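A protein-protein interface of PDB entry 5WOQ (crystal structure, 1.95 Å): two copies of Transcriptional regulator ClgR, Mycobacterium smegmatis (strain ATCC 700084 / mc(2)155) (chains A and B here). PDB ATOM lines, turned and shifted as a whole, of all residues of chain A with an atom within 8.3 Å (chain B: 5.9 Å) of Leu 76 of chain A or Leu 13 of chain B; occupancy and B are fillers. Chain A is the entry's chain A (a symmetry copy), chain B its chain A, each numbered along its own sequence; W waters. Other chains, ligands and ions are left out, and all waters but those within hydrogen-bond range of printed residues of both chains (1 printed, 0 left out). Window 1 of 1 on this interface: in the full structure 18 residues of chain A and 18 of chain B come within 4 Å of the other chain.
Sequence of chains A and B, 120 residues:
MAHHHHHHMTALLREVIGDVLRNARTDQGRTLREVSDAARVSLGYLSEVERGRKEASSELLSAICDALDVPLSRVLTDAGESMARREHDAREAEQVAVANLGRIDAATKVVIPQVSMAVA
Water W1 bridges the backbone carbonyl oxygen of Ser 58 of chain A (2.8 Å) and the backbone NH of Leu 13 of chain B (2.9 Å).
Leu 13 of chain A touches Leu 76 of chain B, and with the chains exchanged Leu 76 of chain A touches Leu 13 of chain B. Leu 76 of chain A touches its own counterpart, Leu 76 of chain B. Leu 76 of chain A touches Ala 79 of chain B, and with the chains exchanged Ala 79 of chain A touches Leu 76 of chain B. Thr 77 of chain A touches Gly 80 of chain B, and with the chains exchanged Gly 80 of chain A touches Thr 77 of chain B.
Of chain B, only Leu 13 (3.3 Å), Leu 76 (3.7 Å), Ala 79 (3.9 Å) and Gly 80 (3.7 Å) come within 4 Å of Leu 76 of chain A. Of chain A, only Ser 58, Leu 61, Leu 72 and Leu 76 come within 4 Å of Leu 13 of chain B. Printed residues of chain A within 4 Å of Leu 12 of chain B: Ser 58. Printed residues of chain B within 4 Å of Thr 77 of chain A: Gly 80 (3.8 Å). Printed residues of chain B within 4 Å of Glu 59 of chain A: Arg 14 and Glu 55. Pro 71 of chain A touches none of the printed residues of chain B.
The backbone NH of Arg 14 of chain B is in hydrogen-bond range of the side-chain hydroxyl of Ser 58 of chain A, at 2.9 Å. The guanidinium group of Arg 14 of chain B lies within salt-bridge range of the side-chain carboxylate of Glu 59 of chain A, at 2.6 Å. OE1 of Glu 55 of chain B sits at hydrogen-bond distance from OG of Ser 58 of chain A, at 2.7 Å.
CB of Ser 58 of chain A touches CB of Leu 12 of chain B, at 3.9 Å. CB of Leu 13 of chain B touches OG of Ser 58 of chain A, at 3.3 Å. Leu 61 of chain A touches Leu 13 of chain B (CD2 to CD2, 3.5 Å). CD2 of Leu 72 of chain A touches N of Leu 13 of chain B, at 3.97 Å. CD2 of Leu 72 of chain A touches CE of Met 83 of chain B, at 3.5 Å. O of Leu 76 of chain A touches O of Leu 76 of chain B, at 3.7 Å. CB of Leu 76 of chain A touches CA of Gly 80 of chain B, at 3.7 Å. OG1 of Thr 77 of chain A touches CA of Gly 80 of chain B, 3.8 Å away. Leu 76 of chain B touches Gly 80 of chain A (CB to CA, 3.7 Å). CA of Gly 80 of chain A touches OG1 of Thr 77 of chain B, 3.8 Å away.
Of the 27 printed residues of chain A, 11 touch a printed residue of chain B.
NH1 of Arg 14 of chain B is in salt-bridge range of OE1 of Glu 55 of chain B. OG1 of Thr 77 of chain A sits at hydrogen-bond distance from O of Ser 73 of chain A (3.1 Å). The backbone NH of Leu 12 of chain B sits at hydrogen-bond distance from the side-chain carboxylate of Glu 15 of chain B (3.0 Å). O of Leu 61 of chain A is in hydrogen-bond range of SG of Cys 65 of chain A.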
ATOM      1  N   LEU A  13     -18.341 -17.740   7.523  1.00  0.00           N
ATOM      2  CA  LEU A  13     -19.772 -17.653   7.268  1.00  0.00           C
ATOM      3  C   LEU A  13     -20.525 -18.857   7.839  1.00  0.00           C
ATOM      4  O   LEU A  13     -21.525 -18.693   8.544  1.00  0.00           O
ATOM      5  CB  LEU A  13     -20.041 -17.522   5.770  1.00  0.00           C
ATOM      6  CG  LEU A  13     -21.559 -17.518   5.555  1.00  0.00           C
ATOM      7  CD1 LEU A  13     -22.141 -16.371   6.324  1.00  0.00           C
ATOM      8  CD2 LEU A  13     -21.968 -17.431   4.095  1.00  0.00           C
ATOM      9  N   VAL A  16     -21.108 -18.836  11.710  1.00  0.00           N
ATOM     10  CA  VAL A  16     -22.082 -17.857  12.185  1.00  0.00           C
ATOM     11  C   VAL A  16     -23.473 -18.225  11.705  1.00  0.00           C
ATOM     12  O   VAL A  16     -24.462 -18.074  12.441  1.00  0.00           O
ATOM     13  CB  VAL A  16     -21.668 -16.438  11.733  1.00  0.00           C
ATOM     14  CG1 VAL A  16     -22.741 -15.429  12.100  1.00  0.00           C
ATOM     15  CG2 VAL A  16     -20.377 -16.058  12.414  1.00  0.00           C
ATOM     16  N   ILE A  17     -23.576 -18.733  10.470  1.00  0.00           N
ATOM     17  CA  ILE A  17     -24.866 -19.221   9.983  1.00  0.00           C
ATOM     18  C   ILE A  17     -25.329 -20.403  10.819  1.00  0.00           C
ATOM     19  O   ILE A  17     -26.516 -20.517  11.150  1.00  0.00           O
ATOM     20  CB  ILE A  17     -24.783 -19.595   8.489  1.00  0.00           C
ATOM     21  CG1 ILE A  17     -24.581 -18.346   7.625  1.00  0.00           C
ATOM     22  CG2 ILE A  17     -26.063 -20.317   8.042  1.00  0.00           C
ATOM     23  CD1 ILE A  17     -25.778 -17.449   7.570  1.00  0.00           C
ATOM     24  N   VAL A  20     -26.897 -19.445  14.107  1.00  0.00           N
ATOM     25  CA  VAL A  20     -28.230 -18.897  13.865  1.00  0.00           C
ATOM     26  C   VAL A  20     -29.219 -20.020  13.608  1.00  0.00           C
ATOM     27  O   VAL A  20     -30.340 -20.005  14.126  1.00  0.00           O
ATOM     28  CB  VAL A  20     -28.190 -17.900  12.689  1.00  0.00           C
ATOM     29  CG1 VAL A  20     -29.604 -17.545  12.247  1.00  0.00           C
ATOM     30  CG2 VAL A  20     -27.421 -16.651  13.083  1.00  0.00           C
ATOM     31  N   LEU A  21     -28.826 -21.019  12.810  1.00  0.00           N
ATOM     32  CA  LEU A  21     -29.748 -22.128  12.538  1.00  0.00           C
ATOM     33  C   LEU A  21     -30.022 -22.946  13.800  1.00  0.00           C
ATOM     34  O   LEU A  21     -31.167 -23.346  14.058  1.00  0.00           O
ATOM     35  CB  LEU A  21     -29.187 -23.026  11.436  1.00  0.00           C
ATOM     36  CG  LEU A  21     -29.021 -22.381  10.052  1.00  0.00           C
ATOM     37  CD1 LEU A  21     -28.530 -23.433   9.061  1.00  0.00           C
ATOM     38  CD2 LEU A  21     -30.302 -21.720   9.556  1.00  0.00           C
ATOM     39  N   GLU A  55     -20.600 -26.817   4.890  1.00  0.00           N
ATOM     40  CA  GLU A  55     -21.324 -25.770   4.175  1.00  0.00           C
ATOM     41  C   GLU A  55     -22.688 -26.287   3.742  1.00  0.00           C
ATOM     42  O   GLU A  55     -22.786 -27.360   3.136  1.00  0.00           O
ATOM     43  CB  GLU A  55     -20.556 -25.314   2.939  1.00  0.00           C
ATOM     44  CG  GLU A  55     -19.152 -24.817   3.194  1.00  0.00           C
ATOM     45  CD  GLU A  55     -19.109 -23.348   3.577  1.00  0.00           C
ATOM     46  OE1 GLU A  55     -18.070 -22.931   4.118  1.00  0.00           O
ATOM     47  OE2 GLU A  55     -20.100 -22.620   3.345  1.00  0.00           O
ATOM     48  N   ALA A  56     -23.738 -25.523   4.031  1.00  0.00           N
ATOM     49  CA  ALA A  56     -25.067 -25.844   3.526  1.00  0.00           C
ATOM     50  C   ALA A  56     -25.291 -25.151   2.189  1.00  0.00           C
ATOM     51  O   ALA A  56     -25.100 -23.938   2.078  1.00  0.00           O
ATOM     52  CB  ALA A  56     -26.149 -25.421   4.524  1.00  0.00           C
ATOM     53  N   SER A  57     -25.684 -25.923   1.171  1.00  0.00           N
ATOM     54  CA  SER A  57     -26.083 -25.333  -0.099  1.00  0.00           C
ATOM     55  C   SER A  57     -27.231 -24.345   0.113  1.00  0.00           C
ATOM     56  O   SER A  57     -27.947 -24.387   1.123  1.00  0.00           O
ATOM     57  CB  SER A  57     -26.504 -26.426  -1.083  1.00  0.00           C
ATOM     58  OG  SER A  57     -27.688 -27.071  -0.627  1.00  0.00           O
ATOM     59  N   SER A  58     -27.397 -23.429  -0.844  1.00  0.00           N
ATOM     60  CA  SER A  58     -28.532 -22.514  -0.747  1.00  0.00           C
ATOM     61  C   SER A  58     -29.841 -23.282  -0.690  1.00  0.00           C
ATOM     62  O   SER A  58     -30.765 -22.906   0.045  1.00  0.00           O
ATOM     63  CB  SER A  58     -28.545 -21.544  -1.927  1.00  0.00           C
ATOM     64  OG  SER A  58     -27.449 -20.646  -1.872  1.00  0.00           O
ATOM     65  N   GLU A  59     -29.934 -24.373  -1.455  1.00  0.00           N
ATOM     66  CA  GLU A  59     -31.165 -25.166  -1.459  1.00  0.00           C
ATOM     67  C   GLU A  59     -31.436 -25.772  -0.085  1.00  0.00           C
ATOM     68  O   GLU A  59     -32.579 -25.769   0.400  1.00  0.00           O
ATOM     69  CB  GLU A  59     -31.074 -26.264  -2.522  1.00  0.00           C
ATOM     70  CG  GLU A  59     -31.156 -25.785  -3.977  1.00  0.00           C
ATOM     71  CD  GLU A  59     -29.832 -25.254  -4.522  1.00  0.00           C
ATOM     72  OE1 GLU A  59     -28.817 -25.254  -3.786  1.00  0.00           O
ATOM     73  OE2 GLU A  59     -29.813 -24.847  -5.703  1.00  0.00           O
ATOM     74  N   LEU A  61     -30.190 -24.686   2.873  1.00  0.00           N
ATOM     75  CA  LEU A  61     -30.509 -23.572   3.758  1.00  0.00           C
ATOM     76  C   LEU A  61     -31.979 -23.181   3.646  1.00  0.00           C
ATOM     77  O   LEU A  61     -32.648 -22.927   4.657  1.00  0.00           O
ATOM     78  CB  LEU A  61     -29.622 -22.375   3.420  1.00  0.00           C
ATOM     79  CG  LEU A  61     -29.324 -21.342   4.480  1.00  0.00           C
ATOM     80  CD1 LEU A  61     -28.835 -21.998   5.756  1.00  0.00           C
ATOM     81  CD2 LEU A  61     -28.255 -20.457   3.911  1.00  0.00           C
ATOM     82  N   SER A  62     -32.496 -23.100   2.426  1.00  0.00           N
ATOM     83  CA  SER A  62     -33.896 -22.721   2.265  1.00  0.00           C
ATOM     84  C   SER A  62     -34.813 -23.786   2.845  1.00  0.00           C
ATOM     85  O   SER A  62     -35.845 -23.463   3.442  1.00  0.00           O
ATOM     86  CB  SER A  62     -34.219 -22.476   0.793  1.00  0.00           C
ATOM     87  OG  SER A  62     -35.610 -22.232   0.629  1.00  0.00           O
ATOM     88  N   CYS A  65     -34.730 -23.277   6.638  1.00  0.00           N
ATOM     89  CA  CYS A  65     -35.564 -22.124   6.979  1.00  0.00           C
ATOM     90  C   CYS A  65     -37.051 -22.456   6.872  1.00  0.00           C
ATOM     91  O   CYS A  65     -37.853 -22.024   7.704  1.00  0.00           O
ATOM     92  CB  CYS A  65     -35.218 -20.936   6.080  1.00  0.00           C
ATOM     93  SG  CYS A  65     -33.559 -20.271   6.504  1.00  0.00           S
ATOM     94  N   VAL A  70     -38.625 -19.694   9.444  1.00  0.00           N
ATOM     95  CA  VAL A  70     -37.788 -18.517   9.639  1.00  0.00           C
ATOM     96  C   VAL A  70     -37.431 -17.978   8.259  1.00  0.00           C
ATOM     97  O   VAL A  70     -37.013 -18.753   7.400  1.00  0.00           O
ATOM     98  CB  VAL A  70     -36.512 -18.828  10.443  1.00  0.00           C
ATOM     99  CG1 VAL A  70     -35.565 -17.647  10.433  1.00  0.00           C
ATOM    100  CG2 VAL A  70     -36.870 -19.205  11.878  1.00  0.00           C
ATOM    101  N   PRO A  71     -37.618 -16.690   7.994  1.00  0.00           N
ATOM    102  CA  PRO A  71     -37.229 -16.151   6.691  1.00  0.00           C
ATOM    103  C   PRO A  71     -35.716 -16.130   6.555  1.00  0.00           C
ATOM    104  O   PRO A  71     -34.997 -15.758   7.488  1.00  0.00           O
ATOM    105  CB  PRO A  71     -37.793 -14.723   6.701  1.00  0.00           C
ATOM    106  CG  PRO A  71     -38.698 -14.647   7.895  1.00  0.00           C
ATOM    107  CD  PRO A  71     -38.211 -15.663   8.866  1.00  0.00           C
ATOM    108  N   LEU A  72     -35.246 -16.514   5.367  1.00  0.00           N
ATOM    109  CA  LEU A  72     -33.820 -16.440   5.069  1.00  0.00           C
ATOM    110  C   LEU A  72     -33.283 -15.025   5.238  1.00  0.00           C
ATOM    111  O   LEU A  72     -32.111 -14.847   5.576  1.00  0.00           O
ATOM    112  CB  LEU A  72     -33.560 -16.939   3.649  1.00  0.00           C
ATOM    113  CG  LEU A  72     -32.097 -17.002   3.212  1.00  0.00           C
ATOM    114  CD1 LEU A  72     -31.315 -17.927   4.128  1.00  0.00           C
ATOM    115  CD2 LEU A  72     -32.009 -17.480   1.780  1.00  0.00           C
ATOM    116  N   SER A  73     -34.111 -14.006   5.006  1.00  0.00           N
ATOM    117  CA  SER A  73     -33.650 -12.643   5.233  1.00  0.00           C
ATOM    118  C   SER A  73     -33.228 -12.445   6.684  1.00  0.00           C
ATOM    119  O   SER A  73     -32.213 -11.801   6.962  1.00  0.00           O
ATOM    120  CB  SER A  73     -34.744 -11.645   4.858  1.00  0.00           C
ATOM    121  OG  SER A  73     -35.878 -11.786   5.715  1.00  0.00           O
ATOM    122  N   ARG A  74     -34.010 -12.980   7.629  1.00  0.00           N
ATOM    123  CA  ARG A  74     -33.686 -12.814   9.041  1.00  0.00           C
ATOM    124  C   ARG A  74     -32.463 -13.627   9.433  1.00  0.00           C
ATOM    125  O   ARG A  74     -31.690 -13.205  10.300  1.00  0.00           O
ATOM    126  CB  ARG A  74     -34.883 -13.214   9.907  1.00  0.00           C
ATOM    127  CG  ARG A  74     -34.748 -12.801  11.361  1.00  0.00           C
ATOM    128  CD  ARG A  74     -36.022 -13.110  12.121  1.00  0.00           C
ATOM    129  NE  ARG A  74     -35.941 -14.369  12.856  1.00  0.00           N
ATOM    130  CZ  ARG A  74     -36.985 -15.164  13.078  1.00  0.00           C
ATOM    131  NH1 ARG A  74     -38.182 -14.842  12.599  1.00  0.00           N
ATOM    132  NH2 ARG A  74     -36.830 -16.286  13.766  1.00  0.00           N
ATOM    133  N   VAL A  75     -32.286 -14.804   8.831  1.00  0.00           N
ATOM    134  CA  VAL A  75     -31.081 -15.589   9.076  1.00  0.00           C
ATOM    135  C   VAL A  75     -29.846 -14.797   8.649  1.00  0.00           C
ATOM    136  O   VAL A  75     -28.850 -14.724   9.380  1.00  0.00           O
ATOM    137  CB  VAL A  75     -31.172 -16.938   8.344  1.00  0.00           C
ATOM    138  CG1 VAL A  75     -29.810 -17.614   8.288  1.00  0.00           C
ATOM    139  CG2 VAL A  75     -32.213 -17.842   9.028  1.00  0.00           C
ATOM    140  N   LEU A  76     -29.912 -14.171   7.470  1.00  0.00           N
ATOM    141  CA  LEU A  76     -28.770 -13.408   6.958  1.00  0.00           C
ATOM    142  C   LEU A  76     -28.497 -12.171   7.805  1.00  0.00           C
ATOM    143  O   LEU A  76     -27.340 -11.870   8.115  1.00  0.00           O
ATOM    144  CB  LEU A  76     -29.010 -13.015   5.506  1.00  0.00           C
ATOM    145  CG  LEU A  76     -29.027 -14.180   4.513  1.00  0.00           C
ATOM    146  CD1 LEU A  76     -29.638 -13.707   3.194  1.00  0.00           C
ATOM    147  CD2 LEU A  76     -27.620 -14.639   4.322  1.00  0.00           C
ATOM    148  N   THR A  77     -29.545 -11.431   8.169  1.00  0.00           N
ATOM    149  CA  THR A  77     -29.376 -10.233   8.984  1.00  0.00           C
ATOM    150  C   THR A  77     -28.835 -10.582  10.364  1.00  0.00           C
ATOM    151  O   THR A  77     -27.957  -9.899  10.901  1.00  0.00           O
ATOM    152  CB  THR A  77     -30.715  -9.507   9.112  1.00  0.00           C
ATOM    153  OG1 THR A  77     -31.121  -8.997   7.834  1.00  0.00           O
ATOM    154  CG2 THR A  77     -30.616  -8.368  10.115  1.00  0.00           C
ATOM    155  N   ASP A  78     -29.364 -11.647  10.962  1.00  0.00           N
ATOM    156  CA  ASP A  78     -28.873 -12.028  12.280  1.00  0.00           C
ATOM    157  C   ASP A  78     -27.431 -12.496  12.210  1.00  0.00           C
ATOM    158  O   ASP A  78     -26.638 -12.212  13.111  1.00  0.00           O
ATOM    159  CB  ASP A  78     -29.746 -13.129  12.874  1.00  0.00           C
ATOM    160  CG  ASP A  78     -31.062 -12.608  13.410  1.00  0.00           C
ATOM    161  OD1 ASP A  78     -31.289 -11.381  13.416  1.00  0.00           O
ATOM    162  OD2 ASP A  78     -31.870 -13.454  13.835  1.00  0.00           O
ATOM    163  N   ALA A  79     -27.085 -13.225  11.146  1.00  0.00           N
ATOM    164  CA  ALA A  79     -25.709 -13.661  10.951  1.00  0.00           C
ATOM    165  C   ALA A  79     -24.787 -12.476  10.753  1.00  0.00           C
ATOM    166  O   ALA A  79     -23.659 -12.477  11.255  1.00  0.00           O
ATOM    167  CB  ALA A  79     -25.600 -14.588   9.741  1.00  0.00           C
ATOM    168  N   GLY A  80     -25.246 -11.470  10.002  1.00  0.00           N
ATOM    169  CA  GLY A  80     -24.448 -10.264   9.807  1.00  0.00           C
ATOM    170  C   GLY A  80     -24.216  -9.499  11.097  1.00  0.00           C
ATOM    171  O   GLY A  80     -23.104  -9.020  11.355  1.00  0.00           O
ATOM    172  N   GLU A  81     -25.262  -9.373  11.931  1.00  0.00           N
ATOM    173  CA  GLU A  81     -25.105  -8.717  13.230  1.00  0.00           C
ATOM    174  C   GLU A  81     -24.137  -9.489  14.114  1.00  0.00           C
ATOM    175  O   GLU A  81     -23.305  -8.892  14.806  1.00  0.00           O
ATOM    176  CB  GLU A  81     -26.460  -8.573  13.937  1.00  0.00           C
ATOM    177  CG  GLU A  81     -27.406  -7.570  13.285  1.00  0.00           C
ATOM    178  CD  GLU A  81     -28.814  -7.570  13.877  1.00  0.00           C
ATOM    179  OE1 GLU A  81     -29.125  -8.412  14.754  1.00  0.00           O
ATOM    180  OE2 GLU A  81     -29.619  -6.718  13.449  1.00  0.00           O
ATOM    181  N   SER A  82     -24.230 -10.818  14.104  1.00  0.00           N
ATOM    182  CA  SER A  82     -23.283 -11.615  14.871  1.00  0.00           C
ATOM    183  C   SER A  82     -21.874 -11.442  14.333  1.00  0.00           C
ATOM    184  O   SER A  82     -20.922 -11.263  15.100  1.00  0.00           O
ATOM    185  CB  SER A  82     -23.678 -13.093  14.840  1.00  0.00           C
ATOM    186  OG  SER A  82     -22.713 -13.869  15.530  1.00  0.00           O
ATOM    187  N   MET A  83     -21.724 -11.504  13.013  1.00  0.00           N
ATOM    188  CA  MET A  83     -20.402 -11.365  12.414  1.00  0.00           C
ATOM    189  C   MET A  83     -19.823  -9.979  12.688  1.00  0.00           C
ATOM    190  O   MET A  83     -18.608  -9.833  12.883  1.00  0.00           O
ATOM    191  CB  MET A  83     -20.502 -11.659  10.911  1.00  0.00           C
ATOM    192  CG  MET A  83     -19.191 -11.543  10.178  1.00  0.00           C
ATOM    193  SD  MET A  83     -18.095 -12.852  10.708  1.00  0.00           S
ATOM    194  CE  MET A  83     -18.859 -14.250   9.893  1.00  0.00           C
ATOM    195  N   ALA B  11     -35.798 -16.720  -4.232  1.00  0.00           N
ATOM    196  CA  ALA B  11     -34.411 -16.362  -4.496  1.00  0.00           C
ATOM    197  C   ALA B  11     -33.487 -17.128  -3.559  1.00  0.00           C
ATOM    198  O   ALA B  11     -33.781 -17.302  -2.373  1.00  0.00           O
ATOM    199  CB  ALA B  11     -34.208 -14.854  -4.329  1.00  0.00           C
ATOM    200  N   LEU B  12     -32.372 -17.602  -4.101  1.00  0.00           N
ATOM    201  CA  LEU B  12     -31.446 -18.441  -3.355  1.00  0.00           C
ATOM    202  C   LEU B  12     -30.359 -17.591  -2.708  1.00  0.00           C
ATOM    203  O   LEU B  12     -29.931 -16.576  -3.265  1.00  0.00           O
ATOM    204  CB  LEU B  12     -30.810 -19.488  -4.279  1.00  0.00           C
ATOM    205  CG  LEU B  12     -31.835 -20.477  -4.872  1.00  0.00           C
ATOM    206  CD1 LEU B  12     -31.310 -21.026  -6.186  1.00  0.00           C
ATOM    207  CD2 LEU B  12     -32.178 -21.598  -3.892  1.00  0.00           C
ATOM    208  N   LEU B  13     -29.894 -18.033  -1.534  1.00  0.00           N
ATOM    209  CA  LEU B  13     -28.799 -17.334  -0.876  1.00  0.00           C
ATOM    210  C   LEU B  13     -27.698 -16.947  -1.866  1.00  0.00           C
ATOM    211  O   LEU B  13     -27.260 -15.793  -1.895  1.00  0.00           O
ATOM    212  CB  LEU B  13     -28.221 -18.188   0.251  1.00  0.00           C
ATOM    213  CG  LEU B  13     -27.024 -17.442   0.851  1.00  0.00           C
ATOM    214  CD1 LEU B  13     -27.500 -16.112   1.351  1.00  0.00           C
ATOM    215  CD2 LEU B  13     -26.327 -18.202   1.966  1.00  0.00           C
ATOM    216  N   ARG B  14     -27.276 -17.882  -2.727  1.00  0.00           N
ATOM    217  CA  ARG B  14     -26.117 -17.607  -3.585  1.00  0.00           C
ATOM    218  C   ARG B  14     -26.408 -16.543  -4.647  1.00  0.00           C
ATOM    219  O   ARG B  14     -25.487 -15.839  -5.075  1.00  0.00           O
ATOM    220  CB  ARG B  14     -25.608 -18.893  -4.247  1.00  0.00           C
ATOM    221  CG  ARG B  14     -26.573 -19.556  -5.226  1.00  0.00           C
ATOM    222  CD  ARG B  14     -25.929 -20.784  -5.866  1.00  0.00           C
ATOM    223  NE  ARG B  14     -26.867 -21.506  -6.710  1.00  0.00           N
ATOM    224  CZ  ARG B  14     -27.474 -22.628  -6.338  1.00  0.00           C
ATOM    225  NH1 ARG B  14     -27.227 -23.148  -5.139  1.00  0.00           N
ATOM    226  NH2 ARG B  14     -28.327 -23.222  -7.152  1.00  0.00           N
ATOM    227  N   GLU B  15     -27.665 -16.402  -5.080  1.00  0.00           N
ATOM    228  CA  GLU B  15     -28.002 -15.337  -6.028  1.00  0.00           C
ATOM    229  C   GLU B  15     -27.940 -13.961  -5.369  1.00  0.00           C
ATOM    230  O   GLU B  15     -27.456 -12.994  -5.974  1.00  0.00           O
ATOM    231  CB  GLU B  15     -29.391 -15.575  -6.617  1.00  0.00           C
ATOM    232  CG  GLU B  15     -29.456 -16.747  -7.598  1.00  0.00           C
ATOM    233  CD  GLU B  15     -30.868 -17.295  -7.769  1.00  0.00           C
ATOM    234  OE1 GLU B  15     -31.743 -16.975  -6.939  1.00  0.00           O
ATOM    235  OE2 GLU B  15     -31.101 -18.044  -8.736  1.00  0.00           O
ATOM    236  N   VAL B  16     -28.447 -13.848  -4.138  1.00  0.00           N
ATOM    237  CA  VAL B  16     -28.441 -12.559  -3.451  1.00  0.00           C
ATOM    238  C   VAL B  16     -27.039 -12.218  -2.985  1.00  0.00           C
ATOM    239  O   VAL B  16     -26.612 -11.054  -3.046  1.00  0.00           O
ATOM    240  CB  VAL B  16     -29.453 -12.580  -2.282  1.00  0.00           C
ATOM    241  CG1 VAL B  16     -29.359 -11.298  -1.474  1.00  0.00           C
ATOM    242  CG2 VAL B  16     -30.849 -12.715  -2.837  1.00  0.00           C
ATOM    243  N   ILE B  17     -26.287 -13.229  -2.528  1.00  0.00           N
ATOM    244  CA  ILE B  17     -24.887 -12.999  -2.173  1.00  0.00           C
ATOM    245  C   ILE B  17     -24.096 -12.586  -3.403  1.00  0.00           C
ATOM    246  O   ILE B  17     -23.241 -11.693  -3.335  1.00  0.00           O
ATOM    247  CB  ILE B  17     -24.275 -14.252  -1.513  1.00  0.00           C
ATOM    248  CG1 ILE B  17     -24.902 -14.504  -0.138  1.00  0.00           C
ATOM    249  CG2 ILE B  17     -22.756 -14.089  -1.353  1.00  0.00           C
ATOM    250  CD1 ILE B  17     -24.521 -13.491   0.896  1.00  0.00           C
ATOM    251  N   GLY B  18     -24.362 -13.240  -4.541  1.00  0.00           N
ATOM    252  CA  GLY B  18     -23.598 -12.964  -5.750  1.00  0.00           C
ATOM    253  C   GLY B  18     -23.761 -11.532  -6.221  1.00  0.00           C
ATOM    254  O   GLY B  18     -22.785 -10.881  -6.616  1.00  0.00           O
ATOM    255  N   GLU B  55     -22.041 -22.049  -5.613  1.00  0.00           N
ATOM    256  CA  GLU B  55     -21.903 -21.727  -4.196  1.00  0.00           C
ATOM    257  C   GLU B  55     -20.446 -21.426  -3.874  1.00  0.00           C
ATOM    258  O   GLU B  55     -19.555 -22.210  -4.219  1.00  0.00           O
ATOM    259  CB  GLU B  55     -22.372 -22.882  -3.318  1.00  0.00           C
ATOM    260  CG  GLU B  55     -23.792 -23.340  -3.554  1.00  0.00           C
ATOM    261  CD  GLU B  55     -24.808 -22.530  -2.769  1.00  0.00           C
ATOM    262  OE1 GLU B  55     -25.995 -22.601  -3.132  1.00  0.00           O
ATOM    263  OE2 GLU B  55     -24.428 -21.830  -1.803  1.00  0.00           O
ATOM    264  N   LEU B  76     -23.339  -9.860   4.537  1.00  0.00           N
ATOM    265  CA  LEU B  76     -24.489 -10.605   5.058  1.00  0.00           C
ATOM    266  C   LEU B  76     -25.681  -9.691   5.314  1.00  0.00           C
ATOM    267  O   LEU B  76     -26.818 -10.040   4.979  1.00  0.00           O
ATOM    268  CB  LEU B  76     -24.102 -11.343   6.334  1.00  0.00           C
ATOM    269  CG  LEU B  76     -23.100 -12.485   6.145  1.00  0.00           C
ATOM    270  CD1 LEU B  76     -22.523 -12.877   7.505  1.00  0.00           C
ATOM    271  CD2 LEU B  76     -23.822 -13.628   5.514  1.00  0.00           C
ATOM    272  N   THR B  77     -25.446  -8.530   5.925  1.00  0.00           N
ATOM    273  CA  THR B  77     -26.527  -7.591   6.205  1.00  0.00           C
ATOM    274  C   THR B  77     -27.143  -7.066   4.915  1.00  0.00           C
ATOM    275  O   THR B  77     -28.366  -6.942   4.791  1.00  0.00           O
ATOM    276  CB  THR B  77     -25.994  -6.430   7.044  1.00  0.00           C
ATOM    277  OG1 THR B  77     -25.605  -6.901   8.343  1.00  0.00           O
ATOM    278  CG2 THR B  77     -27.045  -5.340   7.184  1.00  0.00           C
ATOM    279  N   ALA B  79     -27.126  -8.561   2.013  1.00  0.00           N
ATOM    280  CA  ALA B  79     -27.837  -9.680   1.410  1.00  0.00           C
ATOM    281  C   ALA B  79     -29.167  -9.910   2.097  1.00  0.00           C
ATOM    282  O   ALA B  79     -30.161 -10.222   1.436  1.00  0.00           O
ATOM    283  CB  ALA B  79     -27.004 -10.958   1.490  1.00  0.00           C
ATOM    284  N   GLY B  80     -29.191  -9.786   3.428  1.00  0.00           N
ATOM    285  CA  GLY B  80     -30.441  -9.933   4.165  1.00  0.00           C
ATOM    286  C   GLY B  80     -31.458  -8.861   3.817  1.00  0.00           C
ATOM    287  O   GLY B  80     -32.650  -9.152   3.656  1.00  0.00           O
ATOM    288  N   MET B  83     -32.716  -9.745   0.420  1.00  0.00           N
ATOM    289  CA  MET B  83     -33.604 -10.898   0.500  1.00  0.00           C
ATOM    290  C   MET B  83     -34.940 -10.514   1.133  1.00  0.00           C
ATOM    291  O   MET B  83     -35.993 -11.038   0.744  1.00  0.00           O
ATOM    292  CB  MET B  83     -32.900 -12.018   1.277  1.00  0.00           C
ATOM    293  CG  MET B  83     -33.727 -13.269   1.429  1.00  0.00           C
ATOM    294  SD  MET B  83     -33.933 -14.043  -0.169  1.00  0.00           S
ATOM    295  CE  MET B  83     -32.288 -14.706  -0.410  1.00  0.00           C
HETATM  296  O   HOH W   1     -31.117 -20.148  -0.010  1.00  0.00           O
